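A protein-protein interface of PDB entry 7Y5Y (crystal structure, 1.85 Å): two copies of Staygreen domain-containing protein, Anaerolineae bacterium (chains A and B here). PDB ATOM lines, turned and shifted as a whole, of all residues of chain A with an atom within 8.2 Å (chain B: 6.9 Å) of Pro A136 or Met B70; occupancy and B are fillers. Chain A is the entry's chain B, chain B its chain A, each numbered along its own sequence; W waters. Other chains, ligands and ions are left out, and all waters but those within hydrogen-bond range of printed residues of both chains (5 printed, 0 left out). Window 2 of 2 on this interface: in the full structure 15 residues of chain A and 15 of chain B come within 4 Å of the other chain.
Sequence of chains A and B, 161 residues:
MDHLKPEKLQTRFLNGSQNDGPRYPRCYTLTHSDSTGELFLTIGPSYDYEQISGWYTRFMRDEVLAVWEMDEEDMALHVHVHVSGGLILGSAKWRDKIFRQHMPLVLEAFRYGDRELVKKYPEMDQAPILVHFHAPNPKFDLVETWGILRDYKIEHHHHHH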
ATOM      1  N   HIS A  82       9.774 -14.527  13.437  1.00  0.00           N
ATOM      2  CA  HIS A  82      10.564 -13.611  12.617  1.00  0.00           C
ATOM      3  C   HIS A  82      10.638 -14.178  11.205  1.00  0.00           C
ATOM      4  O   HIS A  82      11.506 -14.997  10.898  1.00  0.00           O
ATOM      5  CB  HIS A  82      11.972 -13.451  13.181  1.00  0.00           C
ATOM      6  CG  HIS A  82      12.792 -12.402  12.494  1.00  0.00           C
ATOM      7  ND1 HIS A  82      12.632 -11.055  12.741  1.00  0.00           N
ATOM      8  CD2 HIS A  82      13.791 -12.500  11.581  1.00  0.00           C
ATOM      9  CE1 HIS A  82      13.500 -10.369  12.014  1.00  0.00           C
ATOM     10  NE2 HIS A  82      14.209 -11.223  11.295  1.00  0.00           N
ATOM     11  N   VAL A  83       9.727 -13.715  10.351  1.00  0.00           N
ATOM     12  CA  VAL A  83       9.682 -14.223   8.986  1.00  0.00           C
ATOM     13  C   VAL A  83      10.833 -13.646   8.178  1.00  0.00           C
ATOM     14  O   VAL A  83      11.553 -14.373   7.483  1.00  0.00           O
ATOM     15  CB  VAL A  83       8.319 -13.920   8.347  1.00  0.00           C
ATOM     16  CG1 VAL A  83       8.411 -14.022   6.823  1.00  0.00           C
ATOM     17  CG2 VAL A  83       7.274 -14.862   8.913  1.00  0.00           C
ATOM     18  N   SER A  84      11.061 -12.342   8.293  1.00  0.00           N
ATOM     19  CA  SER A  84      12.116 -11.694   7.525  1.00  0.00           C
ATOM     20  C   SER A  84      12.703 -10.519   8.293  1.00  0.00           C
ATOM     21  O   SER A  84      12.087  -9.971   9.215  1.00  0.00           O
ATOM     22  CB  SER A  84      11.603 -11.220   6.154  1.00  0.00           C
ATOM     23  OG  SER A  84      12.637 -10.590   5.423  1.00  0.00           O
ATOM     24  N   GLY A  85      13.902 -10.122   7.882  1.00  0.00           N
ATOM     25  CA  GLY A  85      14.537  -8.948   8.437  1.00  0.00           C
ATOM     26  C   GLY A  85      15.932  -9.201   8.964  1.00  0.00           C
ATOM     27  O   GLY A  85      16.155 -10.124   9.751  1.00  0.00           O
ATOM     28  N   GLY A  86      16.881  -8.380   8.531  1.00  0.00           N
ATOM     29  CA  GLY A  86      18.244  -8.544   8.973  1.00  0.00           C
ATOM     30  C   GLY A  86      18.917  -9.704   8.268  1.00  0.00           C
ATOM     31  O   GLY A  86      18.377 -10.347   7.356  1.00  0.00           O
ATOM     32  N   ILE A  88      19.991 -13.103   8.000  1.00  0.00           N
ATOM     33  CA  ILE A  88      19.449 -14.362   8.509  1.00  0.00           C
ATOM     34  C   ILE A  88      19.425 -15.359   7.360  1.00  0.00           C
ATOM     35  O   ILE A  88      19.488 -14.987   6.190  1.00  0.00           O
ATOM     36  CB  ILE A  88      18.001 -14.225   9.063  1.00  0.00           C
ATOM     37  CG1 ILE A  88      17.084 -13.716   7.942  1.00  0.00           C
ATOM     38  CG2 ILE A  88      17.963 -13.272  10.224  1.00  0.00           C
ATOM     39  CD1 ILE A  88      15.631 -13.507   8.337  1.00  0.00           C
ATOM     40  N   ALA A  92      12.362 -14.673   2.888  1.00  0.00           N
ATOM     41  CA  ALA A  92      11.073 -14.414   3.545  1.00  0.00           C
ATOM     42  C   ALA A  92      10.010 -15.455   3.158  1.00  0.00           C
ATOM     43  O   ALA A  92       9.256 -15.931   4.019  1.00  0.00           O
ATOM     44  CB  ALA A  92      10.600 -12.993   3.216  1.00  0.00           C
ATOM     45  N   PHE A 133       3.336 -12.707  12.244  1.00  0.00           N
ATOM     46  CA  PHE A 133       4.436 -13.031  11.326  1.00  0.00           C
ATOM     47  C   PHE A 133       5.178 -11.742  10.999  1.00  0.00           C
ATOM     48  O   PHE A 133       4.748 -10.955  10.149  1.00  0.00           O
ATOM     49  CB  PHE A 133       3.883 -13.713  10.070  1.00  0.00           C
ATOM     50  CG  PHE A 133       3.138 -14.981  10.380  1.00  0.00           C
ATOM     51  CD1 PHE A 133       1.789 -14.940  10.719  1.00  0.00           C
ATOM     52  CD2 PHE A 133       3.783 -16.213  10.376  1.00  0.00           C
ATOM     53  CE1 PHE A 133       1.095 -16.099  11.048  1.00  0.00           C
ATOM     54  CE2 PHE A 133       3.086 -17.381  10.707  1.00  0.00           C
ATOM     55  CZ  PHE A 133       1.740 -17.316  11.040  1.00  0.00           C
ATOM     56  N   HIS A 134       6.304 -11.505  11.680  1.00  0.00           N
ATOM     57  CA  HIS A 134       7.034 -10.250  11.524  1.00  0.00           C
ATOM     58  C   HIS A 134       7.873 -10.211  10.246  1.00  0.00           C
ATOM     59  O   HIS A 134       8.700 -11.100  10.016  1.00  0.00           O
ATOM     60  CB  HIS A 134       7.960 -10.026  12.719  1.00  0.00           C
ATOM     61  CG  HIS A 134       7.237  -9.740  13.995  1.00  0.00           C
ATOM     62  ND1 HIS A 134       6.930  -8.459  14.388  1.00  0.00           N
ATOM     63  CD2 HIS A 134       6.819 -10.556  14.991  1.00  0.00           C
ATOM     64  CE1 HIS A 134       6.309  -8.497  15.557  1.00  0.00           C
ATOM     65  NE2 HIS A 134       6.242  -9.756  15.950  1.00  0.00           N
ATOM     66  N   ALA A 135       7.733  -9.129   9.476  1.00  0.00           N
ATOM     67  CA  ALA A 135       8.552  -8.912   8.285  1.00  0.00           C
ATOM     68  C   ALA A 135       8.531  -7.440   7.930  1.00  0.00           C
ATOM     69  O   ALA A 135       7.551  -6.746   8.231  1.00  0.00           O
ATOM     70  CB  ALA A 135       8.040  -9.740   7.098  1.00  0.00           C
ATOM     71  N   PRO A 136       9.570  -6.932   7.269  1.00  0.00           N
ATOM     72  CA  PRO A 136       9.511  -5.537   6.828  1.00  0.00           C
ATOM     73  C   PRO A 136       8.511  -5.329   5.708  1.00  0.00           C
ATOM     74  O   PRO A 136       7.902  -4.259   5.633  1.00  0.00           O
ATOM     75  CB  PRO A 136      10.957  -5.230   6.391  1.00  0.00           C
ATOM     76  CG  PRO A 136      11.582  -6.557   6.175  1.00  0.00           C
ATOM     77  CD  PRO A 136      10.914  -7.514   7.109  1.00  0.00           C
ATOM     78  N   ASN A 137       8.316  -6.336   4.857  1.00  0.00           N
ATOM     79  CA  ASN A 137       7.414  -6.298   3.705  1.00  0.00           C
ATOM     80  C   ASN A 137       5.957  -6.455   4.121  1.00  0.00           C
ATOM     81  O   ASN A 137       5.611  -7.436   4.785  1.00  0.00           O
ATOM     82  CB  ASN A 137       7.796  -7.405   2.721  1.00  0.00           C
ATOM     83  CG  ASN A 137       7.007  -7.354   1.427  1.00  0.00           C
ATOM     84  OD1 ASN A 137       6.305  -6.388   1.144  1.00  0.00           O
ATOM     85  ND2 ASN A 137       7.202  -8.377   0.581  1.00  0.00           N
ATOM     86  N   PRO A 138       5.084  -5.527   3.728  1.00  0.00           N
ATOM     87  CA  PRO A 138       3.642  -5.695   3.977  1.00  0.00           C
ATOM     88  C   PRO A 138       3.094  -7.039   3.543  1.00  0.00           C
ATOM     89  O   PRO A 138       2.178  -7.559   4.186  1.00  0.00           O
ATOM     90  CB  PRO A 138       3.034  -4.544   3.164  1.00  0.00           C
ATOM     91  CG  PRO A 138       4.055  -3.471   3.271  1.00  0.00           C
ATOM     92  CD  PRO A 138       5.406  -4.168   3.260  1.00  0.00           C
ATOM     93  N   LYS A 139       3.641  -7.625   2.470  1.00  0.00           N
ATOM     94  CA  LYS A 139       3.173  -8.925   1.994  1.00  0.00           C
ATOM     95  C   LYS A 139       3.241 -10.006   3.060  1.00  0.00           C
ATOM     96  O   LYS A 139       2.373 -10.884   3.112  1.00  0.00           O
ATOM     97  CB  LYS A 139       3.984  -9.349   0.754  1.00  0.00           C
ATOM     98  CG  LYS A 139       3.325 -10.462  -0.045  1.00  0.00           C
ATOM     99  CD  LYS A 139       4.316 -11.172  -0.986  1.00  0.00           C
ATOM    100  CE  LYS A 139       3.877 -12.616  -1.281  1.00  0.00           C
ATOM    101  NZ  LYS A 139       2.408 -12.724  -1.543  1.00  0.00           N
ATOM    102  N   PHE A 140       4.270  -9.981   3.916  1.00  0.00           N
ATOM    103  CA  PHE A 140       4.451 -11.037   4.907  1.00  0.00           C
ATOM    104  C   PHE A 140       4.175 -10.604   6.339  1.00  0.00           C
ATOM    105  O   PHE A 140       4.001 -11.474   7.200  1.00  0.00           O
ATOM    106  CB  PHE A 140       5.877 -11.586   4.835  1.00  0.00           C
ATOM    107  CG  PHE A 140       6.209 -12.135   3.489  1.00  0.00           C
ATOM    108  CD1 PHE A 140       5.719 -13.365   3.089  1.00  0.00           C
ATOM    109  CD2 PHE A 140       6.911 -11.366   2.594  1.00  0.00           C
ATOM    110  CE1 PHE A 140       6.006 -13.852   1.821  1.00  0.00           C
ATOM    111  CE2 PHE A 140       7.197 -11.847   1.320  1.00  0.00           C
ATOM    112  CZ  PHE A 140       6.730 -13.086   0.945  1.00  0.00           C
ATOM    113  N   ASP A 141       4.135  -9.301   6.603  1.00  0.00           N
ATOM    114  CA  ASP A 141       3.860  -8.775   7.942  1.00  0.00           C
ATOM    115  C   ASP A 141       2.390  -8.875   8.339  1.00  0.00           C
ATOM    116  O   ASP A 141       1.628  -7.921   8.164  1.00  0.00           O
ATOM    117  CB  ASP A 141       4.370  -7.336   8.014  1.00  0.00           C
ATOM    118  CG  ASP A 141       4.524  -6.838   9.462  1.00  0.00           C
ATOM    119  OD1 ASP A 141       4.785  -7.663  10.354  1.00  0.00           O
ATOM    120  OD2 ASP A 141       4.473  -5.607   9.667  1.00  0.00           O
ATOM    121  N   ARG B  23      19.761   7.115   5.991  1.00  0.00           N
ATOM    122  CA  ARG B  23      18.463   6.515   5.703  1.00  0.00           C
ATOM    123  C   ARG B  23      18.059   5.490   6.751  1.00  0.00           C
ATOM    124  O   ARG B  23      16.863   5.267   6.977  1.00  0.00           O
ATOM    125  CB  ARG B  23      18.485   5.843   4.332  1.00  0.00           C
ATOM    126  CG  ARG B  23      18.407   6.792   3.169  1.00  0.00           C
ATOM    127  CD  ARG B  23      18.513   6.022   1.874  1.00  0.00           C
ATOM    128  NE  ARG B  23      17.180   5.840   1.316  1.00  0.00           N
ATOM    129  CZ  ARG B  23      16.889   5.041   0.295  1.00  0.00           C
ATOM    130  NH1 ARG B  23      17.847   4.355  -0.321  1.00  0.00           N
ATOM    131  NH2 ARG B  23      15.633   4.940  -0.112  1.00  0.00           N
ATOM    132  N   TYR B  24      19.030   4.849   7.380  1.00  0.00           N
ATOM    133  CA  TYR B  24      18.785   3.736   8.286  1.00  0.00           C
ATOM    134  C   TYR B  24      19.952   3.677   9.255  1.00  0.00           C
ATOM    135  O   TYR B  24      21.108   3.798   8.826  1.00  0.00           O
ATOM    136  CB  TYR B  24      18.640   2.423   7.506  1.00  0.00           C
ATOM    137  CG  TYR B  24      18.306   1.206   8.340  1.00  0.00           C
ATOM    138  CD1 TYR B  24      16.996   0.935   8.740  1.00  0.00           C
ATOM    139  CD2 TYR B  24      19.307   0.328   8.741  1.00  0.00           C
ATOM    140  CE1 TYR B  24      16.697  -0.190   9.506  1.00  0.00           C
ATOM    141  CE2 TYR B  24      19.016  -0.798   9.515  1.00  0.00           C
ATOM    142  CZ  TYR B  24      17.714  -1.048   9.891  1.00  0.00           C
ATOM    143  OH  TYR B  24      17.424  -2.157  10.648  1.00  0.00           O
ATOM    144  N   TRP B  68      11.647   3.149  10.108  1.00  0.00           N
ATOM    145  CA  TRP B  68      11.959   2.718   8.749  1.00  0.00           C
ATOM    146  C   TRP B  68      12.615   1.348   8.816  1.00  0.00           C
ATOM    147  O   TRP B  68      13.595   1.163   9.547  1.00  0.00           O
ATOM    148  CB  TRP B  68      12.897   3.724   8.107  1.00  0.00           C
ATOM    149  CG  TRP B  68      12.215   4.907   7.542  1.00  0.00           C
ATOM    150  CD1 TRP B  68      12.192   6.168   8.063  1.00  0.00           C
ATOM    151  CD2 TRP B  68      11.465   4.954   6.332  1.00  0.00           C
ATOM    152  NE1 TRP B  68      11.471   7.005   7.241  1.00  0.00           N
ATOM    153  CE2 TRP B  68      11.012   6.281   6.170  1.00  0.00           C
ATOM    154  CE3 TRP B  68      11.140   4.002   5.355  1.00  0.00           C
ATOM    155  CZ2 TRP B  68      10.239   6.681   5.072  1.00  0.00           C
ATOM    156  CZ3 TRP B  68      10.369   4.398   4.271  1.00  0.00           C
ATOM    157  CH2 TRP B  68       9.942   5.728   4.135  1.00  0.00           C
ATOM    158  N   GLU B  69      12.089   0.384   8.063  1.00  0.00           N
ATOM    159  CA  GLU B  69      12.597  -0.979   8.112  1.00  0.00           C
ATOM    160  C   GLU B  69      13.154  -1.346   6.738  1.00  0.00           C
ATOM    161  O   GLU B  69      12.620  -0.903   5.722  1.00  0.00           O
ATOM    162  CB  GLU B  69      11.507  -1.932   8.511  1.00  0.00           C
ATOM    163  CG  GLU B  69      11.150  -1.774  10.019  1.00  0.00           C
ATOM    164  CD  GLU B  69      10.285  -2.874  10.559  1.00  0.00           C
ATOM    165  OE1 GLU B  69       9.986  -3.820   9.809  1.00  0.00           O
ATOM    166  OE2 GLU B  69       9.915  -2.807  11.759  1.00  0.00           O
ATOM    167  N   MET B  70      14.248  -2.122   6.724  1.00  0.00           N
ATOM    168  CA  MET B  70      14.897  -2.589   5.487  1.00  0.00           C
ATOM    169  C   MET B  70      14.364  -3.949   5.081  1.00  0.00           C
ATOM    170  O   MET B  70      14.337  -4.875   5.895  1.00  0.00           O
ATOM    171  CB  MET B  70      16.412  -2.739   5.643  1.00  0.00           C
ATOM    172  CG  MET B  70      17.171  -1.547   6.104  1.00  0.00           C
ATOM    173  SD  MET B  70      17.082  -0.274   4.854  1.00  0.00           S
ATOM    174  CE  MET B  70      17.684  -1.147   3.387  1.00  0.00           C
ATOM    175  N   ASP B  71      14.026  -4.095   3.806  1.00  0.00           N
ATOM    176  CA  ASP B  71      13.687  -5.392   3.233  1.00  0.00           C
ATOM    177  C   ASP B  71      14.770  -5.605   2.173  1.00  0.00           C
ATOM    178  O   ASP B  71      14.620  -5.173   1.030  1.00  0.00           O
ATOM    179  CB  ASP B  71      12.277  -5.395   2.636  1.00  0.00           C
ATOM    180  CG  ASP B  71      11.933  -6.699   1.931  1.00  0.00           C
ATOM    181  OD1 ASP B  71      12.516  -7.757   2.292  1.00  0.00           O
ATOM    182  OD2 ASP B  71      11.096  -6.656   0.999  1.00  0.00           O
ATOM    183  N   GLU B  72      15.880  -6.211   2.584  1.00  0.00           N
ATOM    184  CA  GLU B  72      17.087  -6.263   1.769  1.00  0.00           C
ATOM    185  C   GLU B  72      17.442  -4.854   1.311  1.00  0.00           C
ATOM    186  O   GLU B  72      17.938  -4.061   2.118  1.00  0.00           O
ATOM    187  CB  GLU B  72      16.904  -7.241   0.609  1.00  0.00           C
ATOM    188  CG  GLU B  72      17.018  -8.666   1.128  1.00  0.00           C
ATOM    189  CD  GLU B  72      16.489  -9.721   0.192  1.00  0.00           C
ATOM    190  OE1 GLU B  72      16.828 -10.903   0.428  1.00  0.00           O
ATOM    191  OE2 GLU B  72      15.754  -9.380  -0.762  1.00  0.00           O
ATOM    192  N   GLU B  73      17.182  -4.501   0.053  1.00  0.00           N
ATOM    193  CA  GLU B  73      17.420  -3.121  -0.349  1.00  0.00           C
ATOM    194  C   GLU B  73      16.154  -2.271  -0.392  1.00  0.00           C
ATOM    195  O   GLU B  73      16.248  -1.060  -0.611  1.00  0.00           O
ATOM    196  CB  GLU B  73      18.126  -3.072  -1.710  1.00  0.00           C
ATOM    197  CG  GLU B  73      19.497  -3.735  -1.694  1.00  0.00           C
ATOM    198  N   ASP B  74      14.987  -2.866  -0.183  1.00  0.00           N
ATOM    199  CA  ASP B  74      13.722  -2.151  -0.188  1.00  0.00           C
ATOM    200  C   ASP B  74      13.416  -1.610   1.211  1.00  0.00           C
ATOM    201  O   ASP B  74      13.965  -2.076   2.212  1.00  0.00           O
ATOM    202  CB  ASP B  74      12.611  -3.079  -0.661  1.00  0.00           C
ATOM    203  CG  ASP B  74      12.760  -3.454  -2.127  1.00  0.00           C
ATOM    204  OD1 ASP B  74      13.242  -2.600  -2.910  1.00  0.00           O
ATOM    205  OD2 ASP B  74      12.445  -4.612  -2.480  1.00  0.00           O
ATOM    206  N   MET B  75      12.526  -0.615   1.269  1.00  0.00           N
ATOM    207  CA  MET B  75      12.238   0.109   2.505  1.00  0.00           C
ATOM    208  C   MET B  75      10.737   0.166   2.763  1.00  0.00           C
ATOM    209  O   MET B  75       9.922   0.163   1.831  1.00  0.00           O
ATOM    210  CB  MET B  75      12.854   1.517   2.437  1.00  0.00           C
ATOM    211  CG  MET B  75      14.378   1.482   2.478  1.00  0.00           C
ATOM    212  SD  MET B  75      15.142   2.983   3.114  1.00  0.00           S
ATOM    213  CE  MET B  75      15.461   2.621   4.845  1.00  0.00           C
ATOM    214  N   ALA B  76      10.371   0.207   4.047  1.00  0.00           N
ATOM    215  CA  ALA B  76       8.968   0.331   4.410  1.00  0.00           C
ATOM    216  C   ALA B  76       8.889   1.028   5.758  1.00  0.00           C
ATOM    217  O   ALA B  76       9.674   0.720   6.666  1.00  0.00           O
ATOM    218  CB  ALA B  76       8.258  -1.031   4.491  1.00  0.00           C
ATOM    219  N   LEU B  77       7.930   1.950   5.884  1.00  0.00           N
ATOM    220  CA  LEU B  77       7.744   2.714   7.118  1.00  0.00           C
ATOM    221  C   LEU B  77       6.691   2.035   7.988  1.00  0.00           C
ATOM    222  O   LEU B  77       5.522   1.958   7.597  1.00  0.00           O
ATOM    223  CB  LEU B  77       7.344   4.152   6.801  1.00  0.00           C
ATOM    224  CG  LEU B  77       7.168   5.069   8.034  1.00  0.00           C
ATOM    225  CD1 LEU B  77       8.462   5.137   8.830  1.00  0.00           C
ATOM    226  CD2 LEU B  77       6.716   6.475   7.632  1.00  0.00           C
ATOM    227  N   HIS B  78       7.099   1.558   9.178  1.00  0.00           N
ATOM    228  CA  HIS B  78       6.212   0.853  10.100  1.00  0.00           C
ATOM    229  C   HIS B  78       5.779   1.835  11.189  1.00  0.00           C
ATOM    230  O   HIS B  78       6.603   2.275  11.997  1.00  0.00           O
ATOM    231  CB  HIS B  78       6.903  -0.372  10.703  1.00  0.00           C
ATOM    232  CG  HIS B  78       7.085  -1.512   9.745  1.00  0.00           C
ATOM    233  ND1 HIS B  78       6.708  -2.799  10.056  1.00  0.00           N
ATOM    234  CD2 HIS B  78       7.578  -1.560   8.475  1.00  0.00           C
ATOM    235  CE1 HIS B  78       6.964  -3.594   9.027  1.00  0.00           C
ATOM    236  NE2 HIS B  78       7.480  -2.866   8.053  1.00  0.00           N
ATOM    237  N   PRO B 128       5.992   1.716   0.948  1.00  0.00           N
ATOM    238  CA  PRO B 128       4.680   1.499   1.562  1.00  0.00           C
ATOM    239  C   PRO B 128       4.709   1.951   3.010  1.00  0.00           C
ATOM    240  O   PRO B 128       5.727   1.851   3.697  1.00  0.00           O
ATOM    241  CB  PRO B 128       4.487  -0.013   1.473  1.00  0.00           C
ATOM    242  CG  PRO B 128       5.915  -0.540   1.414  1.00  0.00           C
ATOM    243  CD  PRO B 128       6.716   0.463   0.695  1.00  0.00           C
ATOM    244  N   LEU B 130       3.037   1.155   6.598  1.00  0.00           N
ATOM    245  CA  LEU B 130       2.309   0.064   7.202  1.00  0.00           C
ATOM    246  C   LEU B 130       1.967   0.498   8.628  1.00  0.00           C
ATOM    247  O   LEU B 130       2.865   0.905   9.368  1.00  0.00           O
ATOM    248  CB  LEU B 130       3.166  -1.191   7.125  1.00  0.00           C
ATOM    249  CG  LEU B 130       2.641  -2.538   7.566  1.00  0.00           C
ATOM    250  CD1 LEU B 130       1.478  -2.709   6.561  1.00  0.00           C
ATOM    251  CD2 LEU B 130       3.666  -3.602   7.280  1.00  0.00           C
HETATM  252  O   HOH W   1      14.215 -12.319   1.962  1.00  0.00           O
HETATM  253  O   HOH W   2      16.922  -5.995   7.033  1.00  0.00           O
HETATM  254  O   HOH W   3       9.658  -6.126  10.733  1.00  0.00           O
HETATM  255  O   HOH W   4      10.150  -9.474   1.611  1.00  0.00           O
HETATM  256  O   HOH W   5      10.017  -8.956   4.105  1.00  0.00           O
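Ser A84 touches none of the printed residues of chain B. Printed residues of chain B within 4 Å of Ala A135: His B78. Of chain B, only Glu B69, Met B70, Asp B71, Ala B76 and His B78 come within 4 Å of Pro A136. Printed residues of chain B within 4 Å of Pro A138: Pro B128 and Leu B130. Of the printed residues of chain A, Glu B69 touches Pro A136 (3.5 Å). Of chain A, only Pro A136 (3.2 Å) comes within 4 Å of Met B70. Of the printed residues of chain A, Asp B71 touches Pro A136 (3.8 Å) and Asn A137 (3.8 Å). Glu B72 touches none of the printed residues of chain A. Of the printed residues of chain A, Leu B130 touches Pro A138 and Asp A141. The nearest residue of chain B that does not touch Pro A136 is Leu B130 (4.6 Å). The nearest residue of chain A that does not touch Met B70 is Gly A85 (4.8 Å). The nearest printed residue of chain A that does not touch His B78 is Asn A137 (4.8 Å).
His B78 touches Ala A135 (CE1 to O, 3.3 Å). CA of Pro A136 touches OE1 of Glu B69, at 3.5 Å. Pro A136 touches Met B70 (CG to O, 3.2 Å). CG of Pro A136 touches CB of Asp B71 (3.8 Å). Ala B76 touches Pro A136. Asn A137 touches Asp B71. Pro A138 touches Pro B128 (CG to CB, 3.9 Å). Pro A138 touches Leu B130. CE1 of His B78 touches OD2 of Asp A141, at 3.3 Å. OD2 of Asp A141 touches CD2 of Leu B130, at 3.2 Å.
No position is printed for both chains.
Printed residues of chain A that touch a printed residue of chain B: Ala A135, Pro A136, Asn A137, Pro A138 and Asp A141. Of the 15 printed residues of chain B, 7 touch a printed residue of chain A. Among the printed residues, 11 pairs touch across the chains. Among the printed residues, no Asp or Glu carboxylate lies within 4 Å of a Lys or Arg side-chain nitrogen of the other chain.
O of Ala B76 sits at hydrogen-bond distance from N of Glu B69 (2.8 Å). NE2 of His B78 sits close to OE1 of Glu B69, 3.2 Å away. N of Leu B77 sits at hydrogen-bond distance from O of Pro B128, 3.1 Å away. O of Leu B77 lies within hydrogen-bond range of N of Leu B130 (2.8 Å). The side-chain carboxylate (OD1) of Asp A141 lies within hydrogen-bond range of the backbone NH (N) of Ala A135. OD1 of Asn A137 sits close to N of Lys A139 (3.2 Å).
O of Pro A136 is in hydrogen-bond range of NE2 of His B78, at 2.8 Å.
Water W3 lies within hydrogen-bond range of the side-chain carboxylate (OE1) of Glu B69 (2.5 Å) and the backbone carbonyl oxygen (O) of Ala A135 (3.3 Å). Water W2 bridges the backbone NH of Gly A86 (2.8 Å) and the backbone carbonyl oxygen of Met B70 (3.0 Å). Water W4 lies within hydrogen-bond range of the side-chain carboxylate of Asp B71 (3.0 Å) and the side-chain amide nitrogen of Asn A137 (3.3 Å). Water W1 lies within hydrogen-bond range of N of Ala A92 (3.1 Å) and OE1 of Glu B72 (3.3 Å). Water W5 lies within hydrogen-bond range of N of Asn A137 (3.2 Å), OD1 of Asp B71 (3.3 Å) and OG of Ser A84 (3.4 Å).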
